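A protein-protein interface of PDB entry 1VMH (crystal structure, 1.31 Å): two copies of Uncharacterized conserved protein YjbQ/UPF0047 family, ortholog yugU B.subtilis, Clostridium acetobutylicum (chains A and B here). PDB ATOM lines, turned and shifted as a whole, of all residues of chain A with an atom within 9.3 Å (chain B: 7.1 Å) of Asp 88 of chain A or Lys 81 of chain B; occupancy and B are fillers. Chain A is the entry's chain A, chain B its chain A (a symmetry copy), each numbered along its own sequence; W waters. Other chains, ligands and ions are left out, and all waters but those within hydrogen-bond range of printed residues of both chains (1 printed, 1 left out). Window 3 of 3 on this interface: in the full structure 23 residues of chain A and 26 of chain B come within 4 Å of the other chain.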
ATOM      1  N   VAL A  82      -4.705  16.519  18.645  1.00  0.00           N
ATOM      2  CA  VAL A  82      -5.255  16.423  19.986  1.00  0.00           C
ATOM      3  C   VAL A  82      -5.336  17.785  20.696  1.00  0.00           C
ATOM      4  O   VAL A  82      -6.308  18.056  21.425  1.00  0.00           O
ATOM      5  CB  VAL A  82      -4.429  15.425  20.816  1.00  0.00           C
ATOM      6  CG1 VAL A  82      -4.922  15.386  22.294  1.00  0.00           C
ATOM      7  CG2 VAL A  82      -4.517  14.078  20.183  1.00  0.00           C
ATOM      8  N   PHE A  83      -4.351  18.642  20.443  1.00  0.00           N
ATOM      9  CA  PHE A  83      -4.287  19.984  21.001  1.00  0.00           C
ATOM     10  C   PHE A  83      -4.106  20.983  19.873  1.00  0.00           C
ATOM     11  O   PHE A  83      -2.997  21.459  19.626  1.00  0.00           O
ATOM     12  CB  PHE A  83      -3.114  20.085  21.986  1.00  0.00           C
ATOM     13  CG  PHE A  83      -3.228  19.142  23.124  1.00  0.00           C
ATOM     14  CD1 PHE A  83      -4.157  19.358  24.129  1.00  0.00           C
ATOM     15  CD2 PHE A  83      -2.426  18.010  23.195  1.00  0.00           C
ATOM     16  CE1 PHE A  83      -4.273  18.462  25.168  1.00  0.00           C
ATOM     17  CE2 PHE A  83      -2.550  17.107  24.267  1.00  0.00           C
ATOM     18  CZ  PHE A  83      -3.468  17.344  25.235  1.00  0.00           C
ATOM     19  N   PRO A  84      -5.196  21.293  19.161  1.00  0.00           N
ATOM     20  CA  PRO A  84      -5.115  22.150  17.980  1.00  0.00           C
ATOM     21  C   PRO A  84      -4.808  23.617  18.288  1.00  0.00           C
ATOM     22  O   PRO A  84      -4.940  24.064  19.423  1.00  0.00           O
ATOM     23  CB  PRO A  84      -6.486  21.982  17.322  1.00  0.00           C
ATOM     24  CG  PRO A  84      -7.357  21.447  18.358  1.00  0.00           C
ATOM     25  CD  PRO A  84      -6.557  20.795  19.410  1.00  0.00           C
ATOM     26  N   LYS A  85      -4.367  24.350  17.277  1.00  0.00           N
ATOM     27  CA  LYS A  85      -4.057  25.770  17.450  1.00  0.00           C
ATOM     28  C   LYS A  85      -5.291  26.573  17.861  1.00  0.00           C
ATOM     29  O   LYS A  85      -5.194  27.506  18.649  1.00  0.00           O
ATOM     30  CB  LYS A  85      -3.493  26.351  16.137  1.00  0.00           C
ATOM     31  CG  LYS A  85      -2.126  25.832  15.718  1.00  0.00           C
ATOM     32  CD  LYS A  85      -1.449  26.740  14.693  1.00  0.00           C
ATOM     33  N   VAL A  86      -6.448  26.225  17.291  1.00  0.00           N
ATOM     34  CA  VAL A  86      -7.723  26.884  17.618  1.00  0.00           C
ATOM     35  C   VAL A  86      -8.525  26.014  18.567  1.00  0.00           C
ATOM     36  O   VAL A  86      -8.664  24.791  18.362  1.00  0.00           O
ATOM     37  CB  VAL A  86      -8.565  27.219  16.345  1.00  0.00           C
ATOM     38  CG1 VAL A  86      -9.795  28.012  16.722  1.00  0.00           C
ATOM     39  CG2 VAL A  86      -7.727  27.993  15.338  1.00  0.00           C
ATOM     40  N   GLY A  87      -9.022  26.613  19.638  1.00  0.00           N
ATOM     41  CA  GLY A  87      -9.834  25.867  20.593  1.00  0.00           C
ATOM     42  C   GLY A  87     -10.204  26.698  21.803  1.00  0.00           C
ATOM     43  O   GLY A  87     -10.317  27.933  21.724  1.00  0.00           O
ATOM     44  N   ASP A  88     -10.391  26.006  22.927  1.00  0.00           N
ATOM     45  CA  ASP A  88     -10.824  26.589  24.168  1.00  0.00           C
ATOM     46  C   ASP A  88      -9.611  27.141  24.871  1.00  0.00           C
ATOM     47  O   ASP A  88      -9.063  26.523  25.797  1.00  0.00           O
ATOM     48  CB  ASP A  88     -11.502  25.519  25.035  1.00  0.00           C
ATOM     49  CG  ASP A  88     -12.086  26.076  26.311  1.00  0.00           C
ATOM     50  OD1 ASP A  88     -11.963  27.297  26.553  1.00  0.00           O
ATOM     51  OD2 ASP A  88     -12.666  25.281  27.086  1.00  0.00           O
ATOM     52  N   TYR A  89      -9.161  28.283  24.375  1.00  0.00           N
ATOM     53  CA  TYR A  89      -7.954  28.945  24.854  1.00  0.00           C
ATOM     54  C   TYR A  89      -8.233  30.416  25.116  1.00  0.00           C
ATOM     55  O   TYR A  89      -8.646  31.131  24.213  1.00  0.00           O
ATOM     56  CB  TYR A  89      -6.821  28.843  23.838  1.00  0.00           C
ATOM     57  CG  TYR A  89      -6.473  27.468  23.332  1.00  0.00           C
ATOM     58  CD1 TYR A  89      -5.950  26.522  24.172  1.00  0.00           C
ATOM     59  CD2 TYR A  89      -6.617  27.141  21.991  1.00  0.00           C
ATOM     60  CE1 TYR A  89      -5.575  25.265  23.706  1.00  0.00           C
ATOM     61  CE2 TYR A  89      -6.281  25.906  21.516  1.00  0.00           C
ATOM     62  CZ  TYR A  89      -5.737  24.955  22.381  1.00  0.00           C
ATOM     63  OH  TYR A  89      -5.387  23.687  21.949  1.00  0.00           O
ATOM     64  N   LYS A  90      -7.971  30.863  26.333  1.00  0.00           N
ATOM     65  CA  LYS A  90      -8.077  32.265  26.710  1.00  0.00           C
ATOM     66  C   LYS A  90      -6.856  33.092  26.353  1.00  0.00           C
ATOM     67  O   LYS A  90      -6.976  34.303  26.168  1.00  0.00           O
ATOM     68  CB  LYS A  90      -8.310  32.384  28.217  1.00  0.00           C
ATOM     69  CG  LYS A  90      -9.655  31.878  28.673  1.00  0.00           C
ATOM     70  CD  LYS A  90      -9.899  32.255  30.115  1.00  0.00           C
ATOM     71  N   HIS A  91      -5.693  32.439  26.262  1.00  0.00           N
ATOM     72  CA  HIS A  91      -4.435  33.164  26.169  1.00  0.00           C
ATOM     73  C   HIS A  91      -4.363  34.014  24.921  1.00  0.00           C
ATOM     74  O   HIS A  91      -4.515  33.517  23.813  1.00  0.00           O
ATOM     75  CB  HIS A  91      -3.270  32.211  26.213  1.00  0.00           C
ATOM     76  CG  HIS A  91      -1.934  32.882  26.135  1.00  0.00           C
ATOM     77  ND1 HIS A  91      -1.604  33.969  26.916  1.00  0.00           N
ATOM     78  CD2 HIS A  91      -0.831  32.586  25.416  1.00  0.00           C
ATOM     79  CE1 HIS A  91      -0.354  34.319  26.668  1.00  0.00           C
ATOM     80  NE2 HIS A  91       0.132  33.501  25.759  1.00  0.00           N
ATOM     81  N   SER A  96      -1.278  28.894  23.248  1.00  0.00           N
ATOM     82  CA  SER A  96      -1.435  27.934  24.323  1.00  0.00           C
ATOM     83  C   SER A  96      -1.210  26.484  23.859  1.00  0.00           C
ATOM     84  O   SER A  96      -0.730  25.639  24.630  1.00  0.00           O
ATOM     85  CB  SER A  96      -2.795  28.063  25.017  1.00  0.00           C
ATOM     86  OG  SER A  96      -2.773  29.156  25.908  1.00  0.00           O
ATOM     87  N   HIS A  97      -1.605  26.166  22.631  1.00  0.00           N
ATOM     88  CA  HIS A  97      -1.346  24.803  22.106  1.00  0.00           C
ATOM     89  C   HIS A  97       0.128  24.444  22.271  1.00  0.00           C
ATOM     90  O   HIS A  97       0.501  23.306  22.625  1.00  0.00           O
ATOM     91  CB  HIS A  97      -1.756  24.703  20.637  1.00  0.00           C
ATOM     92  CG  HIS A  97      -0.966  25.581  19.720  1.00  0.00           C
ATOM     93  ND1 HIS A  97      -1.158  26.941  19.663  1.00  0.00           N
ATOM     94  CD2 HIS A  97       0.015  25.303  18.828  1.00  0.00           C
ATOM     95  CE1 HIS A  97      -0.327  27.468  18.780  1.00  0.00           C
ATOM     96  NE2 HIS A  97       0.392  26.496  18.254  1.00  0.00           N
ATOM     97  N   ILE A 100       1.129  23.773  25.894  1.00  0.00           N
ATOM     98  CA  ILE A 100       0.686  22.448  26.328  1.00  0.00           C
ATOM     99  C   ILE A 100       1.654  21.397  25.816  1.00  0.00           C
ATOM    100  O   ILE A 100       2.114  20.535  26.559  1.00  0.00           O
ATOM    101  CB  ILE A 100      -0.721  22.137  25.822  1.00  0.00           C
ATOM    102  CG1 ILE A 100      -1.749  23.034  26.520  1.00  0.00           C
ATOM    103  CG2 ILE A 100      -1.070  20.684  26.038  1.00  0.00           C
ATOM    104  CD1 ILE A 100      -3.033  23.124  25.771  1.00  0.00           C
ATOM    105  N   ARG B  73      -4.429  28.267  32.995  1.00  0.00           N
ATOM    106  CA  ARG B  73      -5.807  27.870  32.818  1.00  0.00           C
ATOM    107  C   ARG B  73      -6.021  27.050  31.538  1.00  0.00           C
ATOM    108  O   ARG B  73      -6.651  25.991  31.555  1.00  0.00           O
ATOM    109  CB  ARG B  73      -6.737  29.085  32.845  1.00  0.00           C
ATOM    110  CG  ARG B  73      -8.184  28.783  32.470  1.00  0.00           C
ATOM    111  CD  ARG B  73      -8.454  28.991  30.979  1.00  0.00           C
ATOM    112  NE  ARG B  73      -9.869  28.715  30.653  1.00  0.00           N
ATOM    113  CZ  ARG B  73     -10.310  28.227  29.499  1.00  0.00           C
ATOM    114  NH1 ARG B  73      -9.490  27.944  28.498  1.00  0.00           N
ATOM    115  NH2 ARG B  73     -11.613  28.025  29.336  1.00  0.00           N
ATOM    116  N   ASP B  74      -5.446  27.517  30.430  1.00  0.00           N
ATOM    117  CA  ASP B  74      -5.542  26.781  29.173  1.00  0.00           C
ATOM    118  C   ASP B  74      -4.980  25.371  29.273  1.00  0.00           C
ATOM    119  O   ASP B  74      -5.542  24.433  28.723  1.00  0.00           O
ATOM    120  CB  ASP B  74      -4.853  27.562  28.048  1.00  0.00           C
ATOM    121  CG  ASP B  74      -5.650  28.792  27.609  1.00  0.00           C
ATOM    122  OD1 ASP B  74      -6.829  28.956  28.046  1.00  0.00           O
ATOM    123  OD2 ASP B  74      -5.096  29.589  26.821  1.00  0.00           O
ATOM    124  N   ILE B  75      -3.876  25.206  29.980  1.00  0.00           N
ATOM    125  CA  ILE B  75      -3.288  23.878  30.119  1.00  0.00           C
ATOM    126  C   ILE B  75      -4.192  22.964  30.936  1.00  0.00           C
ATOM    127  O   ILE B  75      -4.506  21.858  30.518  1.00  0.00           O
ATOM    128  CB  ILE B  75      -1.899  23.937  30.772  1.00  0.00           C
ATOM    129  CG1 ILE B  75      -0.907  24.700  29.876  1.00  0.00           C
ATOM    130  CG2 ILE B  75      -1.334  22.528  31.014  1.00  0.00           C
ATOM    131  CD1 ILE B  75       0.437  25.026  30.526  1.00  0.00           C
ATOM    132  N   LEU B  76      -4.623  23.436  32.098  1.00  0.00           N
ATOM    133  CA  LEU B  76      -5.487  22.632  32.953  1.00  0.00           C
ATOM    134  C   LEU B  76      -6.788  22.270  32.251  1.00  0.00           C
ATOM    135  O   LEU B  76      -7.210  21.122  32.260  1.00  0.00           O
ATOM    136  CB  LEU B  76      -5.775  23.366  34.277  1.00  0.00           C
ATOM    137  CG  LEU B  76      -4.585  23.455  35.215  1.00  0.00           C
ATOM    138  CD1 LEU B  76      -4.869  24.329  36.429  1.00  0.00           C
ATOM    139  CD2 LEU B  76      -4.176  22.083  35.663  1.00  0.00           C
ATOM    140  N   VAL B  77      -7.412  23.254  31.644  1.00  0.00           N
ATOM    141  CA  VAL B  77      -8.685  23.052  31.004  1.00  0.00           C
ATOM    142  C   VAL B  77      -8.569  22.072  29.856  1.00  0.00           C
ATOM    143  O   VAL B  77      -9.413  21.208  29.671  1.00  0.00           O
ATOM    144  CB  VAL B  77      -9.283  24.408  30.504  1.00  0.00           C
ATOM    145  CG1 VAL B  77     -10.403  24.216  29.450  1.00  0.00           C
ATOM    146  CG2 VAL B  77      -9.801  25.243  31.671  1.00  0.00           C
ATOM    147  N   ASN B  78      -7.502  22.184  29.079  1.00  0.00           N
ATOM    148  CA  ASN B  78      -7.364  21.330  27.908  1.00  0.00           C
ATOM    149  C   ASN B  78      -6.862  19.924  28.251  1.00  0.00           C
ATOM    150  O   ASN B  78      -7.275  18.955  27.610  1.00  0.00           O
ATOM    151  CB  ASN B  78      -6.595  22.033  26.795  1.00  0.00           C
ATOM    152  CG  ASN B  78      -7.453  23.081  26.103  1.00  0.00           C
ATOM    153  OD1 ASN B  78      -8.272  22.749  25.219  1.00  0.00           O
ATOM    154  ND2 ASN B  78      -7.350  24.324  26.560  1.00  0.00           N
ATOM    155  N   LEU B  79      -6.013  19.793  29.269  1.00  0.00           N
ATOM    156  CA  LEU B  79      -5.717  18.446  29.788  1.00  0.00           C
ATOM    157  C   LEU B  79      -6.985  17.749  30.303  1.00  0.00           C
ATOM    158  O   LEU B  79      -7.191  16.553  30.064  1.00  0.00           O
ATOM    159  CB  LEU B  79      -4.678  18.510  30.900  1.00  0.00           C
ATOM    160  CG  LEU B  79      -3.247  18.866  30.496  1.00  0.00           C
ATOM    161  CD1 LEU B  79      -2.357  18.943  31.706  1.00  0.00           C
ATOM    162  CD2 LEU B  79      -2.672  17.892  29.440  1.00  0.00           C
ATOM    163  N   ASP B  80      -7.849  18.490  30.997  1.00  0.00           N
ATOM    164  CA  ASP B  80      -9.154  17.972  31.424  1.00  0.00           C
ATOM    165  C   ASP B  80     -10.062  17.579  30.277  1.00  0.00           C
ATOM    166  O   ASP B  80     -10.788  16.579  30.346  1.00  0.00           O
ATOM    167  CB  ASP B  80      -9.849  19.002  32.304  1.00  0.00           C
ATOM    168  CG  ASP B  80     -11.228  18.560  32.744  1.00  0.00           C
ATOM    169  OD1 ASP B  80     -11.351  17.581  33.500  1.00  0.00           O
ATOM    170  OD2 ASP B  80     -12.199  19.217  32.337  1.00  0.00           O
ATOM    171  N   LYS B  81     -10.028  18.353  29.209  1.00  0.00           N
ATOM    172  CA  LYS B  81     -10.873  18.071  28.067  1.00  0.00           C
ATOM    173  C   LYS B  81     -10.490  16.729  27.440  1.00  0.00           C
ATOM    174  O   LYS B  81     -11.340  15.944  27.053  1.00  0.00           O
ATOM    175  CB  LYS B  81     -10.743  19.213  27.059  1.00  0.00           C
ATOM    176  CG  LYS B  81     -11.768  19.201  25.948  1.00  0.00           C
ATOM    177  CD  LYS B  81     -11.579  20.389  24.992  1.00  0.00           C
ATOM    178  CE  LYS B  81     -11.586  21.767  25.687  1.00  0.00           C
ATOM    179  NZ  LYS B  81     -12.936  22.152  26.227  1.00  0.00           N
ATOM    180  N   VAL B  82      -9.191  16.455  27.376  1.00  0.00           N
ATOM    181  CA  VAL B  82      -8.681  15.259  26.729  1.00  0.00           C
ATOM    182  C   VAL B  82      -8.769  14.014  27.626  1.00  0.00           C
ATOM    183  O   VAL B  82      -9.068  12.907  27.138  1.00  0.00           O
ATOM    184  CB  VAL B  82      -7.233  15.495  26.266  1.00  0.00           C
ATOM    185  CG1 VAL B  82      -6.617  14.192  25.672  1.00  0.00           C
ATOM    186  CG2 VAL B  82      -7.218  16.603  25.268  1.00  0.00           C
ATOM    187  N   PHE B  83      -8.559  14.205  28.925  1.00  0.00           N
ATOM    188  CA  PHE B  83      -8.636  13.146  29.919  1.00  0.00           C
ATOM    189  C   PHE B  83      -9.585  13.572  31.026  1.00  0.00           C
ATOM    190  O   PHE B  83      -9.151  14.004  32.094  1.00  0.00           O
ATOM    191  CB  PHE B  83      -7.242  12.869  30.499  1.00  0.00           C
ATOM    192  CG  PHE B  83      -6.262  12.438  29.475  1.00  0.00           C
ATOM    193  CD1 PHE B  83      -6.336  11.172  28.916  1.00  0.00           C
ATOM    194  CD2 PHE B  83      -5.265  13.299  29.034  1.00  0.00           C
ATOM    195  CE1 PHE B  83      -5.437  10.790  27.946  1.00  0.00           C
ATOM    196  CE2 PHE B  83      -4.348  12.892  28.047  1.00  0.00           C
ATOM    197  CZ  PHE B  83      -4.445  11.648  27.518  1.00  0.00           C
ATOM    198  N   PRO B  84     -10.894  13.475  30.769  1.00  0.00           N
ATOM    199  CA  PRO B  84     -11.894  13.967  31.714  1.00  0.00           C
ATOM    200  C   PRO B  84     -12.009  13.139  32.996  1.00  0.00           C
ATOM    201  O   PRO B  84     -11.536  12.008  33.060  1.00  0.00           O
ATOM    202  CB  PRO B  84     -13.192  13.945  30.905  1.00  0.00           C
ATOM    203  CG  PRO B  84     -12.940  13.056  29.780  1.00  0.00           C
ATOM    204  CD  PRO B  84     -11.492  12.942  29.535  1.00  0.00           C
ATOM    205  N   LYS B 101      -2.646  12.488  34.050  1.00  0.00           N
ATOM    206  CA  LYS B 101      -2.067  13.798  33.875  1.00  0.00           C
ATOM    207  C   LYS B 101      -0.747  13.958  34.626  1.00  0.00           C
ATOM    208  O   LYS B 101       0.175  14.622  34.154  1.00  0.00           O
ATOM    209  CB  LYS B 101      -3.069  14.886  34.252  1.00  0.00           C
ATOM    210  CG  LYS B 101      -4.258  14.891  33.307  1.00  0.00           C
ATOM    211  CD  LYS B 101      -5.304  15.977  33.572  1.00  0.00           C
ATOM    212  CE  LYS B 101      -6.047  15.799  34.833  1.00  0.00           C
ATOM    213  NZ  LYS B 101      -7.215  16.819  34.984  1.00  0.00           N
HETATM  214  O   HOH W   1      -9.841  23.288  22.984  1.00  0.00           O
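The side-chain carboxylate (OD1) of Asp 74 of chain B is in salt-bridge range of the guanidinium group (NH1) of Arg 73 of chain B, 2.9 Å away.
The backbone carbonyl oxygen (O) of Asp 74 of chain B lies within hydrogen-bond range of the side-chain amide nitrogen (ND2) of Asn 78 of chain B (2.8 Å).
OH of Tyr 89 of chain A is in hydrogen-bond range of O of Pro 84 of chain A.
Val 82 of chain B touches its own counterpart, Val 82 of chain A.
Phe 83 of chain A touches Val 82 of chain B, but with the chains exchanged Val 82 of chain A does not touch Phe 83 of chain B (6.3 Å).
Of the 16 pairs that touch across the chains among the printed residues, 1 has its exchanged pair printed and touching as well.
The side-chain carboxylate (OD2) of Asp 74 of chain B is in hydrogen-bond range of the side-chain hydroxyl (OG) of Ser 96 of chain A (2.5 Å).
NZ of Lys 81 of chain B is in salt-bridge range of OD2 of Asp 88 of chain A (3.3 Å).
NH2 of Arg 73 of chain B is in salt-bridge range of OD1 of Asp 88 of chain A (2.9 Å).
ND2 of Asn 78 of chain B sits at hydrogen-bond distance from O of Asp 88 of chain A (2.9 Å).
The backbone NH (N) of Lys 90 of chain A sits at hydrogen-bond distance from the side-chain carboxylate (OD1) of Asp 74 of chain B (2.8 Å).
The backbone NH (N) of His 91 of chain A sits at hydrogen-bond distance from the side-chain carboxylate (OD2) of Asp 74 of chain B (3.0 Å).
Val 82 of chain A touches Val 82 of chain B.
CE1 of Phe 83 of chain A touches O of Asn 78 of chain B, 3.9 Å away.
Phe 83 of chain A touches Val 82 of chain B.
Asp 88 of chain A touches Asp 74 of chain B.
Val 77 of chain B touches Asp 88 of chain A.
Tyr 89 of chain A touches Asp 74 of chain B (CA to OD1, 3.4 Å).
Asn 78 of chain B touches Tyr 89 of chain A (ND2 to CE1, 3.5 Å).
Arg 73 of chain B touches Lys 90 of chain A.
Ile 75 of chain B touches Ile 100 of chain A (CG1 to CG1, 3.8 Å).
Ile 100 of chain A touches Asn 78 of chain B (CD1 to CB, 3.9 Å).
Printed residues of chain B within 4 Å of Asp 88 of chain A: Arg 73, Asp 74, Val 77, Asn 78 and Lys 81.
Lys 81 of chain B touches just one residue of chain A: Asp 88 (3.3 Å).
No residue of chain A comes within 4 Å of Asp 80 of chain B.
Of chain A, only Val 82 (3.9 Å) and Phe 83 (3.5 Å) come within 4 Å of Val 82 of chain B.
Of the printed residues of chain B, Phe 83 of chain A touches Asn 78 (3.9 Å) and Val 82 (3.5 Å).
Of the printed residues of chain B, Lys 90 of chain A touches Arg 73 and Asp 74.
Of the printed residues of chain B, Ser 96 of chain A touches Asp 74.
Printed residues of chain B within 4 Å of Ile 100 of chain A: Ile 75 (3.8 Å) and Asn 78 (3.9 Å).
Of the printed residues of chain A, Asp 74 of chain B touches Asp 88, Tyr 89, Lys 90, His 91 and Ser 96.
Phe 83 of chain B touches none of the printed residues of chain A.
Leu 79 of chain B touches none of the printed residues of chain A.
The nearest residue of chain A that does not touch Lys 81 of chain B is Gly 87 of chain A (6.4 Å).
Printed residues of chain A that touch a printed residue of chain B: Val 82, Phe 83, Asp 88, Tyr 89, Lys 90, His 91, Ser 96 and Ile 100.
Hydrophobic or aromatic side chains of chain A that line the printed part of chain B: Val 82, Phe 83, Tyr 89, His 91 and Ile 100.
Hydrophobic or aromatic side chains of chain B that line the printed part of chain A: Ile 75, Val 77 and Val 82.
Among the printed residues, 16 pairs touch across the chains.
Water W1 lies within hydrogen-bond range of N of Asp 88 of chain A and OD1 of Asn 78 of chain B.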
